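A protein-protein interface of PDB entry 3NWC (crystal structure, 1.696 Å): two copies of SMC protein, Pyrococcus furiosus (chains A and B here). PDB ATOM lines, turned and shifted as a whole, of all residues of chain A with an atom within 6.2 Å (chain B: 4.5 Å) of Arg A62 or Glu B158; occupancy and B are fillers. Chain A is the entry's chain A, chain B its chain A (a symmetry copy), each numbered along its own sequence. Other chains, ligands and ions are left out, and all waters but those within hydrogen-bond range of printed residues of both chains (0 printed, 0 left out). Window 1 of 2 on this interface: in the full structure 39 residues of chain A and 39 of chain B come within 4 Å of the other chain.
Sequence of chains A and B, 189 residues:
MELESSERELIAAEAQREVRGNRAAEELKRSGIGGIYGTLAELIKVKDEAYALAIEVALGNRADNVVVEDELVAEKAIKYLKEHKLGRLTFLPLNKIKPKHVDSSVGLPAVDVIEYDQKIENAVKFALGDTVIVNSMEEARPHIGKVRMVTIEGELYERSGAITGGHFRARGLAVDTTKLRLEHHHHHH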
ATOM      1  N   THR A  39      12.086  12.679 -10.004  1.00  0.00           N
ATOM      2  CA  THR A  39      12.557  13.912  -9.391  1.00  0.00           C
ATOM      3  C   THR A  39      12.755  14.999 -10.438  1.00  0.00           C
ATOM      4  O   THR A  39      12.990  14.699 -11.606  1.00  0.00           O
ATOM      5  CB  THR A  39      13.900  13.690  -8.676  1.00  0.00           C
ATOM      6  OG1 THR A  39      14.894  13.326  -9.641  1.00  0.00           O
ATOM      7  CG2 THR A  39      13.784  12.569  -7.641  1.00  0.00           C
ATOM      8  N   LEU A  40      12.678  16.259 -10.025  1.00  0.00           N
ATOM      9  CA  LEU A  40      12.953  17.360 -10.932  1.00  0.00           C
ATOM     10  C   LEU A  40      14.355  17.252 -11.518  1.00  0.00           C
ATOM     11  O   LEU A  40      14.570  17.604 -12.666  1.00  0.00           O
ATOM     12  CB  LEU A  40      12.771  18.713 -10.234  1.00  0.00           C
ATOM     13  CG  LEU A  40      11.324  19.165 -10.106  1.00  0.00           C
ATOM     14  CD1 LEU A  40      11.227  20.497  -9.346  1.00  0.00           C
ATOM     15  CD2 LEU A  40      10.749  19.297 -11.513  1.00  0.00           C
ATOM     16  N   ALA A  41      15.302  16.769 -10.719  1.00  0.00           N
ATOM     17  CA  ALA A  41      16.661  16.557 -11.215  1.00  0.00           C
ATOM     18  C   ALA A  41      16.696  15.604 -12.408  1.00  0.00           C
ATOM     19  O   ALA A  41      17.581  15.710 -13.260  1.00  0.00           O
ATOM     20  CB  ALA A  41      17.572  16.053 -10.098  1.00  0.00           C
ATOM     21  N   ALA A  58      19.610  27.558  -8.074  1.00  0.00           N
ATOM     22  CA  ALA A  58      18.227  28.015  -7.996  1.00  0.00           C
ATOM     23  C   ALA A  58      17.235  26.882  -7.710  1.00  0.00           C
ATOM     24  O   ALA A  58      16.174  27.106  -7.106  1.00  0.00           O
ATOM     25  CB  ALA A  58      17.825  28.791  -9.258  1.00  0.00           C
ATOM     26  N   LEU A  59      17.547  25.677  -8.181  1.00  0.00           N
ATOM     27  CA  LEU A  59      16.722  24.514  -7.858  1.00  0.00           C
ATOM     28  C   LEU A  59      16.931  24.112  -6.406  1.00  0.00           C
ATOM     29  O   LEU A  59      15.979  23.820  -5.689  1.00  0.00           O
ATOM     30  CB  LEU A  59      17.092  23.334  -8.739  1.00  0.00           C
ATOM     31  CG  LEU A  59      16.261  22.949  -9.948  1.00  0.00           C
ATOM     32  CD1 LEU A  59      16.764  21.620 -10.483  1.00  0.00           C
ATOM     33  CD2 LEU A  59      14.799  22.829  -9.553  1.00  0.00           C
ATOM     34  N   GLY A  60      18.188  24.090  -5.976  1.00  0.00           N
ATOM     35  CA  GLY A  60      18.507  23.673  -4.616  1.00  0.00           C
ATOM     36  C   GLY A  60      17.869  22.333  -4.288  1.00  0.00           C
ATOM     37  O   GLY A  60      17.930  21.396  -5.092  1.00  0.00           O
ATOM     38  N   ASN A  61      17.245  22.239  -3.118  1.00  0.00           N
ATOM     39  CA  ASN A  61      16.638  20.983  -2.679  1.00  0.00           C
ATOM     40  C   ASN A  61      15.462  20.557  -3.536  1.00  0.00           C
ATOM     41  O   ASN A  61      15.051  19.399  -3.515  1.00  0.00           O
ATOM     42  CB  ASN A  61      16.176  21.077  -1.224  1.00  0.00           C
ATOM     43  CG  ASN A  61      17.317  20.992  -0.251  1.00  0.00           C
ATOM     44  OD1 ASN A  61      18.413  20.555  -0.601  1.00  0.00           O
ATOM     45  ND2 ASN A  61      17.070  21.403   0.987  1.00  0.00           N
ATOM     46  N   ARG A  62      14.907  21.485  -4.294  1.00  0.00           N
ATOM     47  CA  ARG A  62      13.770  21.148  -5.134  1.00  0.00           C
ATOM     48  C   ARG A  62      14.166  20.090  -6.149  1.00  0.00           C
ATOM     49  O   ARG A  62      13.338  19.330  -6.614  1.00  0.00           O
ATOM     50  CB  ARG A  62      13.218  22.391  -5.835  1.00  0.00           C
ATOM     51  CG  ARG A  62      12.631  23.410  -4.880  1.00  0.00           C
ATOM     52  CD  ARG A  62      11.708  22.740  -3.897  1.00  0.00           C
ATOM     53  NE  ARG A  62      11.087  23.703  -3.000  1.00  0.00           N
ATOM     54  CZ  ARG A  62      10.114  23.408  -2.149  1.00  0.00           C
ATOM     55  NH1 ARG A  62       9.634  22.168  -2.082  1.00  0.00           N
ATOM     56  NH2 ARG A  62       9.613  24.361  -1.376  1.00  0.00           N
ATOM     57  N   ALA A  63      15.452  20.036  -6.481  1.00  0.00           N
ATOM     58  CA  ALA A  63      15.945  19.022  -7.406  1.00  0.00           C
ATOM     59  C   ALA A  63      15.556  17.610  -6.954  1.00  0.00           C
ATOM     60  O   ALA A  63      15.359  16.725  -7.779  1.00  0.00           O
ATOM     61  CB  ALA A  63      17.460  19.131  -7.561  1.00  0.00           C
ATOM     62  N   ASP A  64      15.424  17.407  -5.645  1.00  0.00           N
ATOM     63  CA  ASP A  64      15.096  16.088  -5.095  1.00  0.00           C
ATOM     64  C   ASP A  64      13.590  15.858  -4.922  1.00  0.00           C
ATOM     65  O   ASP A  64      13.164  14.769  -4.533  1.00  0.00           O
ATOM     66  CB  ASP A  64      15.768  15.888  -3.728  1.00  0.00           C
ATOM     67  CG  ASP A  64      17.254  16.192  -3.750  1.00  0.00           C
ATOM     68  OD1 ASP A  64      17.949  15.773  -4.701  1.00  0.00           O
ATOM     69  OD2 ASP A  64      17.725  16.854  -2.803  1.00  0.00           O
ATOM     70  N   ASN A  65      12.784  16.880  -5.191  1.00  0.00           N
ATOM     71  CA  ASN A  65      11.331  16.735  -5.097  1.00  0.00           C
ATOM     72  C   ASN A  65      10.813  15.805  -6.191  1.00  0.00           C
ATOM     73  O   ASN A  65      11.330  15.814  -7.301  1.00  0.00           O
ATOM     74  CB  ASN A  65      10.631  18.086  -5.274  1.00  0.00           C
ATOM     75  CG  ASN A  65      10.795  19.025  -4.087  1.00  0.00           C
ATOM     76  OD1 ASN A  65      10.146  20.076  -4.047  1.00  0.00           O
ATOM     77  ND2 ASN A  65      11.661  18.685  -3.147  1.00  0.00           N
ATOM     78  N   VAL A  66       9.788  15.013  -5.875  1.00  0.00           N
ATOM     79  CA  VAL A  66       9.266  14.004  -6.793  1.00  0.00           C
ATOM     80  C   VAL A  66       7.959  14.489  -7.378  1.00  0.00           C
ATOM     81  O   VAL A  66       7.028  14.791  -6.641  1.00  0.00           O
ATOM     82  CB  VAL A  66       8.987  12.665  -6.074  1.00  0.00           C
ATOM     83  CG1 VAL A  66       8.386  11.652  -7.054  1.00  0.00           C
ATOM     84  CG2 VAL A  66      10.271  12.093  -5.458  1.00  0.00           C
ATOM     85  N   THR A  90       9.564  14.903  -0.649  1.00  0.00           N
ATOM     86  CA  THR A  90       8.651  15.986  -0.945  1.00  0.00           C
ATOM     87  C   THR A  90       8.043  15.733  -2.313  1.00  0.00           C
ATOM     88  O   THR A  90       8.765  15.504  -3.294  1.00  0.00           O
ATOM     89  CB  THR A  90       9.388  17.334  -0.950  1.00  0.00           C
ATOM     90  OG1 THR A  90       9.938  17.564   0.350  1.00  0.00           O
ATOM     91  CG2 THR A  90       8.425  18.472  -1.287  1.00  0.00           C
ATOM     92  N   LEU A  92       5.395  16.764  -5.531  1.00  0.00           N
ATOM     93  CA  LEU A  92       4.785  17.877  -6.262  1.00  0.00           C
ATOM     94  C   LEU A  92       3.622  17.370  -7.126  1.00  0.00           C
ATOM     95  O   LEU A  92       3.844  16.823  -8.207  1.00  0.00           O
ATOM     96  CB  LEU A  92       5.829  18.565  -7.143  1.00  0.00           C
ATOM     97  CG  LEU A  92       7.149  18.943  -6.452  1.00  0.00           C
ATOM     98  CD1 LEU A  92       8.050  19.694  -7.419  1.00  0.00           C
ATOM     99  CD2 LEU A  92       6.881  19.794  -5.224  1.00  0.00           C
ATOM    100  N   PHE A 126       6.788  25.922 -10.685  1.00  0.00           N
ATOM    101  CA  PHE A 126       6.761  26.071  -9.232  1.00  0.00           C
ATOM    102  C   PHE A 126       8.191  26.253  -8.698  1.00  0.00           C
ATOM    103  O   PHE A 126       8.444  27.105  -7.853  1.00  0.00           O
ATOM    104  CB  PHE A 126       6.100  24.870  -8.556  1.00  0.00           C
ATOM    105  CG  PHE A 126       6.627  24.609  -7.173  1.00  0.00           C
ATOM    106  CD1 PHE A 126       6.223  25.397  -6.104  1.00  0.00           C
ATOM    107  CD2 PHE A 126       7.551  23.612  -6.958  1.00  0.00           C
ATOM    108  CE1 PHE A 126       6.730  25.172  -4.844  1.00  0.00           C
ATOM    109  CE2 PHE A 126       8.054  23.384  -5.704  1.00  0.00           C
ATOM    110  CZ  PHE A 126       7.638  24.163  -4.648  1.00  0.00           C
ATOM    111  N   ALA A 127       9.137  25.464  -9.203  1.00  0.00           N
ATOM    112  CA  ALA A 127      10.505  25.531  -8.678  1.00  0.00           C
ATOM    113  C   ALA A 127      11.309  26.725  -9.201  1.00  0.00           C
ATOM    114  O   ALA A 127      12.097  27.332  -8.471  1.00  0.00           O
ATOM    115  CB  ALA A 127      11.255  24.228  -8.984  1.00  0.00           C
ATOM    116  N   GLY B 145      -2.437  23.481  -0.945  1.00  0.00           N
ATOM    117  CA  GLY B 145      -2.211  24.514  -1.941  1.00  0.00           C
ATOM    118  C   GLY B 145      -2.763  25.873  -1.555  1.00  0.00           C
ATOM    119  O   GLY B 145      -2.488  26.872  -2.220  1.00  0.00           O
ATOM    120  N   VAL B 147      -3.239  26.650   2.184  1.00  0.00           N
ATOM    121  CA  VAL B 147      -2.800  26.939   3.547  1.00  0.00           C
ATOM    122  C   VAL B 147      -1.508  26.163   3.827  1.00  0.00           C
ATOM    123  O   VAL B 147      -1.417  24.988   3.478  1.00  0.00           O
ATOM    124  CB  VAL B 147      -3.856  26.497   4.574  1.00  0.00           C
ATOM    125  CG1 VAL B 147      -3.442  26.923   5.978  1.00  0.00           C
ATOM    126  CG2 VAL B 147      -5.235  27.057   4.210  1.00  0.00           C
ATOM    127  N   ARG B 148      -0.511  26.808   4.429  1.00  0.00           N
ATOM    128  CA  ARG B 148       0.664  26.040   4.887  1.00  0.00           C
ATOM    129  C   ARG B 148       0.322  25.323   6.187  1.00  0.00           C
ATOM    130  O   ARG B 148      -0.052  25.956   7.171  1.00  0.00           O
ATOM    131  CB  ARG B 148       1.901  26.923   5.064  1.00  0.00           C
ATOM    132  CG  ARG B 148       3.203  26.129   5.331  1.00  0.00           C
ATOM    133  CD  ARG B 148       4.421  27.047   5.404  1.00  0.00           C
ATOM    134  NE  ARG B 148       5.666  26.356   5.037  1.00  0.00           N
ATOM    135  CZ  ARG B 148       6.546  25.870   5.909  1.00  0.00           C
ATOM    136  NH1 ARG B 148       6.332  25.990   7.212  1.00  0.00           N
ATOM    137  NH2 ARG B 148       7.648  25.267   5.473  1.00  0.00           N
ATOM    138  N   LEU B 156       4.272  17.746   6.252  1.00  0.00           N
ATOM    139  CA  LEU B 156       4.358  19.171   5.908  1.00  0.00           C
ATOM    140  C   LEU B 156       3.677  19.441   4.588  1.00  0.00           C
ATOM    141  O   LEU B 156       3.935  18.755   3.599  1.00  0.00           O
ATOM    142  CB  LEU B 156       5.824  19.615   5.815  1.00  0.00           C
ATOM    143  CG  LEU B 156       6.070  21.052   5.347  1.00  0.00           C
ATOM    144  CD1 LEU B 156       5.512  22.072   6.371  1.00  0.00           C
ATOM    145  CD2 LEU B 156       7.557  21.293   5.113  1.00  0.00           C
ATOM    146  N   TYR B 157       2.805  20.448   4.583  1.00  0.00           N
ATOM    147  CA  TYR B 157       2.093  20.880   3.397  1.00  0.00           C
ATOM    148  C   TYR B 157       2.492  22.325   3.133  1.00  0.00           C
ATOM    149  O   TYR B 157       2.070  23.234   3.848  1.00  0.00           O
ATOM    150  CB  TYR B 157       0.583  20.812   3.635  1.00  0.00           C
ATOM    151  CG  TYR B 157       0.060  19.414   3.854  1.00  0.00           C
ATOM    152  CD1 TYR B 157      -0.619  18.740   2.849  1.00  0.00           C
ATOM    153  CD2 TYR B 157       0.257  18.760   5.064  1.00  0.00           C
ATOM    154  CE1 TYR B 157      -1.087  17.457   3.040  1.00  0.00           C
ATOM    155  CE2 TYR B 157      -0.213  17.479   5.264  1.00  0.00           C
ATOM    156  CZ  TYR B 157      -0.887  16.833   4.254  1.00  0.00           C
ATOM    157  OH  TYR B 157      -1.353  15.554   4.454  1.00  0.00           O
ATOM    158  N   GLU B 158       3.329  22.541   2.132  1.00  0.00           N
ATOM    159  CA  GLU B 158       3.733  23.899   1.815  1.00  0.00           C
ATOM    160  C   GLU B 158       2.545  24.585   1.158  1.00  0.00           C
ATOM    161  O   GLU B 158       1.658  23.924   0.622  1.00  0.00           O
ATOM    162  CB  GLU B 158       4.990  23.898   0.939  1.00  0.00           C
ATOM    163  CG  GLU B 158       6.210  23.322   1.664  1.00  0.00           C
ATOM    164  CD  GLU B 158       7.451  23.254   0.795  1.00  0.00           C
ATOM    165  OE1 GLU B 158       8.003  24.322   0.460  1.00  0.00           O
ATOM    166  OE2 GLU B 158       7.880  22.128   0.458  1.00  0.00           O
ATOM    167  N   ARG B 159       2.490  25.908   1.235  1.00  0.00           N
ATOM    168  CA  ARG B 159       1.330  26.611   0.695  1.00  0.00           C
ATOM    169  C   ARG B 159       1.238  26.398  -0.818  1.00  0.00           C
ATOM    170  O   ARG B 159       0.151  26.438  -1.404  1.00  0.00           O
ATOM    171  CB  ARG B 159       1.405  28.099   1.033  1.00  0.00           C
ATOM    172  CG  ARG B 159       0.125  28.872   0.740  1.00  0.00           C
ATOM    173  CD  ARG B 159       0.246  30.291   1.258  1.00  0.00           C
ATOM    174  NE  ARG B 159      -0.947  31.094   1.016  1.00  0.00           N
ATOM    175  CZ  ARG B 159      -1.310  32.123   1.782  1.00  0.00           C
ATOM    176  NH1 ARG B 159      -0.572  32.448   2.839  1.00  0.00           N
ATOM    177  NH2 ARG B 159      -2.407  32.817   1.502  1.00  0.00           N
ATOM    178  N   SER B 160       2.400  26.159  -1.423  1.00  0.00           N
ATOM    179  CA  SER B 160       2.548  25.909  -2.855  1.00  0.00           C
ATOM    180  C   SER B 160       1.796  24.666  -3.309  1.00  0.00           C
ATOM    181  O   SER B 160       1.432  24.540  -4.477  1.00  0.00           O
ATOM    182  CB  SER B 160       4.030  25.693  -3.169  1.00  0.00           C
ATOM    183  OG  SER B 160       4.504  24.509  -2.522  1.00  0.00           O
ATOM    184  N   GLY B 161       1.608  23.727  -2.392  1.00  0.00           N
ATOM    185  CA  GLY B 161       0.988  22.460  -2.725  1.00  0.00           C
ATOM    186  C   GLY B 161       1.951  21.281  -2.592  1.00  0.00           C
ATOM    187  O   GLY B 161       1.548  20.144  -2.805  1.00  0.00           O
ATOM    188  N   ALA B 162       3.207  21.556  -2.249  1.00  0.00           N
ATOM    189  CA  ALA B 162       4.225  20.506  -2.069  1.00  0.00           C
ATOM    190  C   ALA B 162       3.982  19.749  -0.766  1.00  0.00           C
ATOM    191  O   ALA B 162       3.791  20.361   0.288  1.00  0.00           O
ATOM    192  CB  ALA B 162       5.613  21.110  -2.063  1.00  0.00           C
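The side-chain carboxylate of Glu B158 lies within salt-bridge range of the guanidinium group of Arg A62, 2.4 Å away.
The guanidinium group of Arg A62 lies within hydrogen-bond range of the side-chain amide oxygen of Asn A65 (2.9 Å).
The backbone NH of Val A66 sits at hydrogen-bond distance from the backbone carbonyl oxygen of Thr A90, at 2.8 Å.
N of Leu A92 lies within hydrogen-bond range of O of Val A66 (2.8 Å).
OG of Ser B160 sits at hydrogen-bond distance from N of Ala B162.
Ala B162 touches Thr A90 (CB to CG2, 3.9 Å).
Leu A92 touches Ala B162.
Phe A126 touches Ser B160.
Printed residues of chain B within 4 Å of Thr A90: Ala B162.
Of the printed residues of chain B, Leu A92 touches Ala B162 (3.7 Å).
Of the printed residues of chain A, Glu B158 touches Arg A62.
Of the printed residues of chain A, Ser B160 touches Phe A126 (3.2 Å).
Printed residues of chain A within 4 Å of Ala B162: Thr A90 and Leu A92.
The nearest printed residue of chain A that does not touch Glu B158 is Thr A90 (4.1 Å).
The nearest printed residue of chain A that does not touch Ser B160 is Arg A62 (5.2 Å).
Of the 16 printed residues of chain A, 4 touch a printed residue of chain B.
Hydrophobic or aromatic side chains of chain A within 4 Å of the printed part of chain B: Leu A92 and Phe A126.
Along chain A the printed residues that touch a printed residue of chain B span positions 62 to 126.
Of the 10 printed residues of chain B, 3 touch a printed residue of chain A.
Printed residues of chain B that touch a printed residue of chain A: Glu B158, Ser B160 and Ala B162.
No position is printed for both chains.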
